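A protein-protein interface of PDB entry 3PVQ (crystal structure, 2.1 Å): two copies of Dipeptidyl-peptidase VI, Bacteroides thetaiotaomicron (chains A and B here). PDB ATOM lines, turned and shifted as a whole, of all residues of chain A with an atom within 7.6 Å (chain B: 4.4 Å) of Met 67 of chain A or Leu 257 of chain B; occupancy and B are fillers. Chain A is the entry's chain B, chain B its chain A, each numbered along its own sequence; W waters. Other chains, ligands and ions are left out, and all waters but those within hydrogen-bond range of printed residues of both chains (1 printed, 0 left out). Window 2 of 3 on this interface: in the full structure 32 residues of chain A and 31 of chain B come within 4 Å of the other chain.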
ATOM      1  N   HIS A  17      15.090  -5.375  12.545  1.00  0.00           N
ATOM      2  CA  HIS A  17      16.449  -4.951  12.276  1.00  0.00           C
ATOM      3  C   HIS A  17      17.292  -5.974  11.462  1.00  0.00           C
ATOM      4  O   HIS A  17      18.513  -5.891  11.458  1.00  0.00           O
ATOM      5  CB  HIS A  17      17.164  -4.510  13.570  1.00  0.00           C
ATOM      6  CG  HIS A  17      17.502  -5.600  14.544  1.00  0.00           C
ATOM      7  ND1 HIS A  17      16.974  -5.603  15.823  1.00  0.00           N
ATOM      8  CD2 HIS A  17      18.379  -6.623  14.440  1.00  0.00           C
ATOM      9  CE1 HIS A  17      17.497  -6.656  16.431  1.00  0.00           C
ATOM     10  NE2 HIS A  17      18.336  -7.305  15.638  1.00  0.00           N
ATOM     11  N   ILE A  18      16.655  -6.882  10.758  1.00  0.00           N
ATOM     12  CA  ILE A  18      17.304  -7.821   9.821  1.00  0.00           C
ATOM     13  C   ILE A  18      16.552  -7.686   8.477  1.00  0.00           C
ATOM     14  O   ILE A  18      15.384  -7.293   8.506  1.00  0.00           O
ATOM     15  CB  ILE A  18      17.416  -9.292  10.324  1.00  0.00           C
ATOM     16  CG1 ILE A  18      16.030  -9.915  10.584  1.00  0.00           C
ATOM     17  CG2 ILE A  18      18.346  -9.355  11.577  1.00  0.00           C
ATOM     18  CD1 ILE A  18      16.041 -11.426  10.671  1.00  0.00           C
ATOM     19  N   PHE A  29      10.924 -22.353  16.627  1.00  0.00           N
ATOM     20  CA  PHE A  29      11.313 -22.616  15.228  1.00  0.00           C
ATOM     21  C   PHE A  29      10.578 -23.812  14.620  1.00  0.00           C
ATOM     22  O   PHE A  29      10.375 -23.870  13.407  1.00  0.00           O
ATOM     23  CB  PHE A  29      12.822 -22.879  15.125  1.00  0.00           C
ATOM     24  CG  PHE A  29      13.687 -21.731  15.568  1.00  0.00           C
ATOM     25  CD1 PHE A  29      13.709 -20.536  14.850  1.00  0.00           C
ATOM     26  CD2 PHE A  29      14.467 -21.830  16.714  1.00  0.00           C
ATOM     27  CE1 PHE A  29      14.496 -19.466  15.274  1.00  0.00           C
ATOM     28  CE2 PHE A  29      15.265 -20.762  17.127  1.00  0.00           C
ATOM     29  CZ  PHE A  29      15.271 -19.589  16.404  1.00  0.00           C
ATOM     30  N   TYR A  48       5.830 -10.961  25.209  1.00  0.00           N
ATOM     31  CA  TYR A  48       7.183 -11.490  25.294  1.00  0.00           C
ATOM     32  C   TYR A  48       7.177 -12.732  26.191  1.00  0.00           C
ATOM     33  O   TYR A  48       6.713 -12.674  27.331  1.00  0.00           O
ATOM     34  CB  TYR A  48       8.181 -10.443  25.813  1.00  0.00           C
ATOM     35  CG  TYR A  48       9.587 -10.988  25.912  1.00  0.00           C
ATOM     36  CD1 TYR A  48      10.337 -11.250  24.768  1.00  0.00           C
ATOM     37  CD2 TYR A  48      10.157 -11.279  27.143  1.00  0.00           C
ATOM     38  CE1 TYR A  48      11.621 -11.788  24.849  1.00  0.00           C
ATOM     39  CE2 TYR A  48      11.439 -11.823  27.236  1.00  0.00           C
ATOM     40  CZ  TYR A  48      12.171 -12.064  26.084  1.00  0.00           C
ATOM     41  OH  TYR A  48      13.437 -12.593  26.163  1.00  0.00           O
ATOM     42  N   GLY A  50      10.029 -15.049  25.586  1.00  0.00           N
ATOM     43  CA  GLY A  50      11.388 -15.466  25.241  1.00  0.00           C
ATOM     44  C   GLY A  50      11.513 -15.165  23.762  1.00  0.00           C
ATOM     45  O   GLY A  50      12.587 -14.843  23.239  1.00  0.00           O
ATOM     46  N   TRP A  51      10.347 -15.258  23.103  1.00  0.00           N
ATOM     47  CA  TRP A  51      10.026 -14.894  21.746  1.00  0.00           C
ATOM     48  C   TRP A  51       9.027 -13.720  21.822  1.00  0.00           C
ATOM     49  O   TRP A  51       8.334 -13.563  22.829  1.00  0.00           O
ATOM     50  CB  TRP A  51       9.413 -16.096  21.020  1.00  0.00           C
ATOM     51  CG  TRP A  51      10.407 -17.055  20.442  1.00  0.00           C
ATOM     52  CD1 TRP A  51      11.374 -17.746  21.114  1.00  0.00           C
ATOM     53  CD2 TRP A  51      10.463 -17.504  19.082  1.00  0.00           C
ATOM     54  NE1 TRP A  51      12.071 -18.559  20.241  1.00  0.00           N
ATOM     55  CE2 TRP A  51      11.516 -18.449  18.993  1.00  0.00           C
ATOM     56  CE3 TRP A  51       9.720 -17.210  17.928  1.00  0.00           C
ATOM     57  CZ2 TRP A  51      11.884 -19.047  17.781  1.00  0.00           C
ATOM     58  CZ3 TRP A  51      10.084 -17.803  16.730  1.00  0.00           C
ATOM     59  CH2 TRP A  51      11.140 -18.731  16.669  1.00  0.00           C
ATOM     60  N   TYR A  52       8.998 -12.876  20.803  1.00  0.00           N
ATOM     61  CA  TYR A  52       8.067 -11.752  20.741  1.00  0.00           C
ATOM     62  C   TYR A  52       6.888 -12.082  19.859  1.00  0.00           C
ATOM     63  O   TYR A  52       7.078 -12.575  18.734  1.00  0.00           O
ATOM     64  CB  TYR A  52       8.732 -10.497  20.150  1.00  0.00           C
ATOM     65  CG  TYR A  52       9.730  -9.781  21.025  1.00  0.00           C
ATOM     66  CD1 TYR A  52       9.310  -9.020  22.115  1.00  0.00           C
ATOM     67  CD2 TYR A  52      11.086  -9.760  20.696  1.00  0.00           C
ATOM     68  CE1 TYR A  52      10.217  -8.295  22.884  1.00  0.00           C
ATOM     69  CE2 TYR A  52      12.004  -9.043  21.460  1.00  0.00           C
ATOM     70  CZ  TYR A  52      11.566  -8.322  22.561  1.00  0.00           C
ATOM     71  OH  TYR A  52      12.469  -7.606  23.302  1.00  0.00           O
ATOM     72  N   VAL A  64       8.423 -14.105  16.595  1.00  0.00           N
ATOM     73  CA  VAL A  64       9.825 -14.002  16.179  1.00  0.00           C
ATOM     74  C   VAL A  64      10.722 -14.171  17.395  1.00  0.00           C
ATOM     75  O   VAL A  64      10.313 -13.863  18.516  1.00  0.00           O
ATOM     76  CB  VAL A  64      10.182 -12.675  15.433  1.00  0.00           C
ATOM     77  CG1 VAL A  64       9.479 -12.558  14.093  1.00  0.00           C
ATOM     78  CG2 VAL A  64       9.941 -11.433  16.303  1.00  0.00           C
ATOM     79  N   HIS A  65      11.953 -14.638  17.152  1.00  0.00           N
ATOM     80  CA  HIS A  65      13.014 -14.759  18.136  1.00  0.00           C
ATOM     81  C   HIS A  65      13.333 -13.357  18.679  1.00  0.00           C
ATOM     82  O   HIS A  65      13.192 -12.362  17.956  1.00  0.00           O
ATOM     83  CB  HIS A  65      14.240 -15.397  17.462  1.00  0.00           C
ATOM     84  CG  HIS A  65      15.363 -15.714  18.388  1.00  0.00           C
ATOM     85  ND1 HIS A  65      16.259 -14.742  18.790  1.00  0.00           N
ATOM     86  CD2 HIS A  65      15.727 -16.898  18.935  1.00  0.00           C
ATOM     87  CE1 HIS A  65      17.110 -15.355  19.600  1.00  0.00           C
ATOM     88  NE2 HIS A  65      16.833 -16.653  19.709  1.00  0.00           N
ATOM     89  N   ARG A  66      13.755 -13.279  19.940  1.00  0.00           N
ATOM     90  CA  ARG A  66      14.063 -12.021  20.640  1.00  0.00           C
ATOM     91  C   ARG A  66      15.097 -11.105  19.904  1.00  0.00           C
ATOM     92  O   ARG A  66      14.986  -9.870  19.972  1.00  0.00           O
ATOM     93  CB  ARG A  66      14.588 -12.338  22.054  1.00  0.00           C
ATOM     94  N   MET A  67      16.090 -11.705  19.226  1.00  0.00           N
ATOM     95  CA  MET A  67      17.178 -10.956  18.612  1.00  0.00           C
ATOM     96  C   MET A  67      16.910 -10.350  17.248  1.00  0.00           C
ATOM     97  O   MET A  67      17.812  -9.707  16.732  1.00  0.00           O
ATOM     98  CB  MET A  67      18.419 -11.833  18.498  1.00  0.00           C
ATOM     99  CG  MET A  67      19.630 -11.180  19.143  1.00  0.00           C
ATOM    100  SD  MET A  67      21.111 -12.392  19.430  1.00  0.00           S
ATOM    101  CE  MET A  67      20.243 -13.744  20.563  1.00  0.00           C
ATOM    102  N   VAL A  68      15.721 -10.496  16.657  1.00  0.00           N
ATOM    103  CA  VAL A  68      15.529  -9.939  15.315  1.00  0.00           C
ATOM    104  C   VAL A  68      14.786  -8.581  15.334  1.00  0.00           C
ATOM    105  O   VAL A  68      14.729  -7.903  14.311  1.00  0.00           O
ATOM    106  CB  VAL A  68      14.893 -10.957  14.340  1.00  0.00           C
ATOM    107  CG1 VAL A  68      15.713 -12.258  14.319  1.00  0.00           C
ATOM    108  CG2 VAL A  68      13.428 -11.241  14.681  1.00  0.00           C
ATOM    109  N   ILE A  69      14.258  -8.163  16.474  1.00  0.00           N
ATOM    110  CA  ILE A  69      13.590  -6.871  16.493  1.00  0.00           C
ATOM    111  C   ILE A  69      14.236  -5.990  17.558  1.00  0.00           C
ATOM    112  O   ILE A  69      14.861  -6.496  18.514  1.00  0.00           O
ATOM    113  CB  ILE A  69      12.028  -6.936  16.642  1.00  0.00           C
ATOM    114  CG1 ILE A  69      11.599  -7.344  18.050  1.00  0.00           C
ATOM    115  CG2 ILE A  69      11.329  -7.789  15.519  1.00  0.00           C
ATOM    116  CD1 ILE A  69      10.335  -6.600  18.526  1.00  0.00           C
ATOM    117  N   THR A  70      14.109  -4.663  17.371  1.00  0.00           N
ATOM    118  CA  THR A  70      14.614  -3.725  18.356  1.00  0.00           C
ATOM    119  C   THR A  70      13.392  -3.204  19.119  1.00  0.00           C
ATOM    120  O   THR A  70      12.631  -2.422  18.532  1.00  0.00           O
ATOM    121  CB  THR A  70      15.466  -2.605  17.709  1.00  0.00           C
ATOM    122  OG1 THR A  70      16.607  -3.193  17.089  1.00  0.00           O
ATOM    123  CG2 THR A  70      15.934  -1.569  18.716  1.00  0.00           C
ATOM    124  N   ASP A 131      18.798  -1.117  15.431  1.00  0.00           N
ATOM    125  CA  ASP A 131      19.633  -1.581  16.554  1.00  0.00           C
ATOM    126  C   ASP A 131      20.840  -0.671  16.828  1.00  0.00           C
ATOM    127  O   ASP A 131      21.495  -0.849  17.846  1.00  0.00           O
ATOM    128  CB  ASP A 131      20.155  -3.009  16.285  1.00  0.00           C
ATOM    129  CG  ASP A 131      20.843  -3.108  14.945  1.00  0.00           C
ATOM    130  OD1 ASP A 131      20.140  -3.309  13.933  1.00  0.00           O
ATOM    131  OD2 ASP A 131      22.063  -2.890  14.891  1.00  0.00           O
ATOM    132  N   ARG A 133      23.527  -0.184  14.349  1.00  0.00           N
ATOM    133  CA  ARG A 133      24.596  -0.377  13.356  1.00  0.00           C
ATOM    134  C   ARG A 133      24.565   0.747  12.309  1.00  0.00           C
ATOM    135  O   ARG A 133      23.500   1.265  11.981  1.00  0.00           O
ATOM    136  CB  ARG A 133      24.491  -1.751  12.655  1.00  0.00           C
ATOM    137  CG  ARG A 133      25.065  -2.928  13.441  1.00  0.00           C
ATOM    138  CD  ARG A 133      24.673  -4.252  12.781  1.00  0.00           C
ATOM    139  NE  ARG A 133      23.220  -4.455  12.802  1.00  0.00           N
ATOM    140  CZ  ARG A 133      22.564  -5.284  12.002  1.00  0.00           C
ATOM    141  NH1 ARG A 133      23.219  -6.024  11.117  1.00  0.00           N
ATOM    142  NH2 ARG A 133      21.248  -5.409  12.104  1.00  0.00           N
ATOM    143  N   TYR B 171      18.988 -15.369  10.070  1.00  0.00           N
ATOM    144  CA  TYR B 171      18.848 -16.745  10.487  1.00  0.00           C
ATOM    145  C   TYR B 171      17.528 -17.205   9.912  1.00  0.00           C
ATOM    146  O   TYR B 171      16.550 -16.456   9.894  1.00  0.00           O
ATOM    147  CB  TYR B 171      18.872 -16.867  12.022  1.00  0.00           C
ATOM    148  CG  TYR B 171      18.593 -18.257  12.532  1.00  0.00           C
ATOM    149  CD1 TYR B 171      17.291 -18.751  12.593  1.00  0.00           C
ATOM    150  CD2 TYR B 171      19.626 -19.076  12.985  1.00  0.00           C
ATOM    151  CE1 TYR B 171      17.032 -20.049  13.015  1.00  0.00           C
ATOM    152  CE2 TYR B 171      19.367 -20.354  13.486  1.00  0.00           C
ATOM    153  CZ  TYR B 171      18.067 -20.837  13.491  1.00  0.00           C
ATOM    154  OH  TYR B 171      17.768 -22.076  13.984  1.00  0.00           O
ATOM    155  N   HIS B 255      28.654 -17.328  13.797  1.00  0.00           N
ATOM    156  CA  HIS B 255      27.529 -18.253  13.866  1.00  0.00           C
ATOM    157  C   HIS B 255      26.223 -17.568  13.471  1.00  0.00           C
ATOM    158  O   HIS B 255      26.160 -16.349  13.367  1.00  0.00           O
ATOM    159  CB  HIS B 255      27.409 -18.875  15.291  1.00  0.00           C
ATOM    160  CG  HIS B 255      27.112 -17.902  16.408  1.00  0.00           C
ATOM    161  ND1 HIS B 255      26.197 -18.215  17.403  1.00  0.00           N
ATOM    162  CD2 HIS B 255      27.642 -16.684  16.676  1.00  0.00           C
ATOM    163  CE1 HIS B 255      26.202 -17.183  18.242  1.00  0.00           C
ATOM    164  NE2 HIS B 255      27.049 -16.240  17.842  1.00  0.00           N
ATOM    165  N   ALA B 256      25.183 -18.371  13.268  1.00  0.00           N
ATOM    166  CA  ALA B 256      23.853 -17.863  12.936  1.00  0.00           C
ATOM    167  C   ALA B 256      22.942 -18.071  14.132  1.00  0.00           C
ATOM    168  O   ALA B 256      22.752 -19.201  14.595  1.00  0.00           O
ATOM    169  CB  ALA B 256      23.304 -18.563  11.686  1.00  0.00           C
ATOM    170  N   LEU B 257      22.424 -16.962  14.643  1.00  0.00           N
ATOM    171  CA  LEU B 257      21.490 -16.871  15.752  1.00  0.00           C
ATOM    172  C   LEU B 257      20.866 -15.478  15.652  1.00  0.00           C
ATOM    173  O   LEU B 257      21.534 -14.495  15.955  1.00  0.00           O
ATOM    174  CB  LEU B 257      22.225 -17.134  17.089  1.00  0.00           C
ATOM    175  CG  LEU B 257      21.494 -16.855  18.401  1.00  0.00           C
ATOM    176  CD1 LEU B 257      20.355 -17.800  18.615  1.00  0.00           C
ATOM    177  CD2 LEU B 257      22.436 -16.978  19.552  1.00  0.00           C
ATOM    178  N   GLY B 258      19.648 -15.406  15.111  1.00  0.00           N
ATOM    179  CA  GLY B 258      18.956 -14.141  14.829  1.00  0.00           C
ATOM    180  C   GLY B 258      19.393 -13.728  13.434  1.00  0.00           C
ATOM    181  O   GLY B 258      18.584 -13.648  12.502  1.00  0.00           O
ATOM    182  N   ASP B 259      20.711 -13.564  13.269  1.00  0.00           N
ATOM    183  CA  ASP B 259      21.400 -13.307  11.995  1.00  0.00           C
ATOM    184  C   ASP B 259      22.818 -13.919  12.060  1.00  0.00           C
ATOM    185  O   ASP B 259      23.217 -14.453  13.102  1.00  0.00           O
ATOM    186  CB  ASP B 259      21.435 -11.786  11.672  1.00  0.00           C
ATOM    187  CG  ASP B 259      22.331 -10.902  12.537  1.00  0.00           C
ATOM    188  OD1 ASP B 259      22.895 -11.406  13.506  1.00  0.00           O
ATOM    189  OD2 ASP B 259      22.432  -9.680  12.243  1.00  0.00           O
ATOM    190  N   HIS B 261      26.474 -13.491  12.767  1.00  0.00           N
ATOM    191  CA  HIS B 261      27.285 -12.491  13.463  1.00  0.00           C
ATOM    192  C   HIS B 261      28.480 -13.125  14.185  1.00  0.00           C
ATOM    193  O   HIS B 261      28.552 -14.348  14.345  1.00  0.00           O
ATOM    194  CB  HIS B 261      26.437 -11.639  14.447  1.00  0.00           C
ATOM    195  CG  HIS B 261      25.877 -12.404  15.607  1.00  0.00           C
ATOM    196  ND1 HIS B 261      24.700 -13.121  15.495  1.00  0.00           N
ATOM    197  CD2 HIS B 261      26.359 -12.548  16.865  1.00  0.00           C
ATOM    198  CE1 HIS B 261      24.505 -13.679  16.681  1.00  0.00           C
ATOM    199  NE2 HIS B 261      25.480 -13.368  17.535  1.00  0.00           N
ATOM    200  N   ASP B 273      29.063 -13.619  24.057  1.00  0.00           N
ATOM    201  CA  ASP B 273      27.841 -14.429  24.090  1.00  0.00           C
ATOM    202  C   ASP B 273      27.850 -15.262  25.373  1.00  0.00           C
ATOM    203  O   ASP B 273      28.429 -16.360  25.387  1.00  0.00           O
ATOM    204  CB  ASP B 273      27.779 -15.339  22.852  1.00  0.00           C
ATOM    205  CG  ASP B 273      26.451 -16.072  22.677  1.00  0.00           C
ATOM    206  OD1 ASP B 273      25.767 -16.329  23.698  1.00  0.00           O
ATOM    207  OD2 ASP B 273      26.085 -16.369  21.513  1.00  0.00           O
ATOM    208  N   ASN B 276      25.910 -18.968  25.188  1.00  0.00           N
ATOM    209  CA  ASN B 276      26.649 -20.007  24.466  1.00  0.00           C
ATOM    210  C   ASN B 276      28.035 -20.277  25.097  1.00  0.00           C
ATOM    211  O   ASN B 276      28.436 -21.438  25.139  1.00  0.00           O
ATOM    212  CB  ASN B 276      26.732 -19.713  22.974  1.00  0.00           C
ATOM    213  CG  ASN B 276      25.395 -19.926  22.314  1.00  0.00           C
ATOM    214  OD1 ASN B 276      24.777 -20.990  22.426  1.00  0.00           O
ATOM    215  ND2 ASN B 276      24.865 -18.891  21.706  1.00  0.00           N
HETATM  216  O   HOH W   1      21.452  -8.133  10.235  1.00  0.00           O
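Water W1 lies within hydrogen-bond range of the side-chain carboxylate (OD2) of Asp 259 of chain B and the guanidinium group (NH1) of Arg 133 of chain A.
O of Leu 257 of chain B lies close to ND1 of His 261 of chain B, at 3.5 Å. N of Met 67 of chain A sits at hydrogen-bond distance from ND1 of His 65 of chain A. The guanidinium group (NE) of Arg 133 of chain A is in salt-bridge range of the side-chain carboxylate (OD2) of Asp 131 of chain A, at 2.9 Å. O of Met 67 of chain A is in hydrogen-bond range of NE2 of His 17 of chain A, at 2.7 Å. The backbone NH (N) of Tyr 171 of chain B lies within hydrogen-bond range of the backbone carbonyl oxygen (O) of Gly 258 of chain B, 3.0 Å away. The backbone carbonyl oxygen (O) of Asp 259 of chain B is in hydrogen-bond range of a ring nitrogen (ND1) of His 261 of chain B (3.1 Å).
Ile 18 of chain A touches Gly 258 of chain B. CG2 of Ile 18 of chain A touches CB of Asp 259 of chain B (3.9 Å). Phe 29 of chain A touches Tyr 171 of chain B. Leu 257 of chain B touches His 65 of chain A (CD1 to NE2, 3.9 Å). Leu 257 of chain B touches Met 67 of chain A. Val 68 of chain A touches Gly 258 of chain B (CG1 to O, 3.7 Å).
OD2 of Asp 259 of chain B lies within salt-bridge range of NH1 of Arg 133 of chain A, at 3.9 Å.
Printed residues of chain B within 4 Å of Met 67 of chain A: Leu 257 (3.99 Å). Printed residues of chain A within 4 Å of Leu 257 of chain B: His 65 (3.9 Å) and Met 67 (3.99 Å). No residue of chain A comes within 4 Å of Ala 256 of chain B. Of the printed residues of chain A, Asp 259 of chain B touches Ile 18 and Arg 133. Printed residues of chain B within 4 Å of Arg 133 of chain A: Asp 259 (3.9 Å). Printed residues of chain B within 4 Å of Ile 18 of chain A: Gly 258 (3.8 Å) and Asp 259 (3.9 Å). Printed residues of chain A within 4 Å of Tyr 171 of chain B: Phe 29 (3.4 Å). Ile 69 of chain A touches none of the printed residues of chain B. His 17 of chain A touches none of the printed residues of chain B. The nearest printed residue of chain B that does not touch Arg 133 of chain A is His 261 of chain B (7.3 Å).
Printed residues of chain B that touch a printed residue of chain A: Tyr 171, Leu 257, Gly 258 and Asp 259. Hydrophobic or aromatic side chains of chain B that line the printed part of chain A: Tyr 171 and Leu 257. Hydrophobic or aromatic side chains of chain A within 4 Å of the printed part of chain B: Ile 18, Phe 29, His 65, Met 67 and Val 68.
No position is printed for both chains. Of the 7 pairs that touch across the chains among the printed residues, none has its exchanged pair printed and touching as well.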
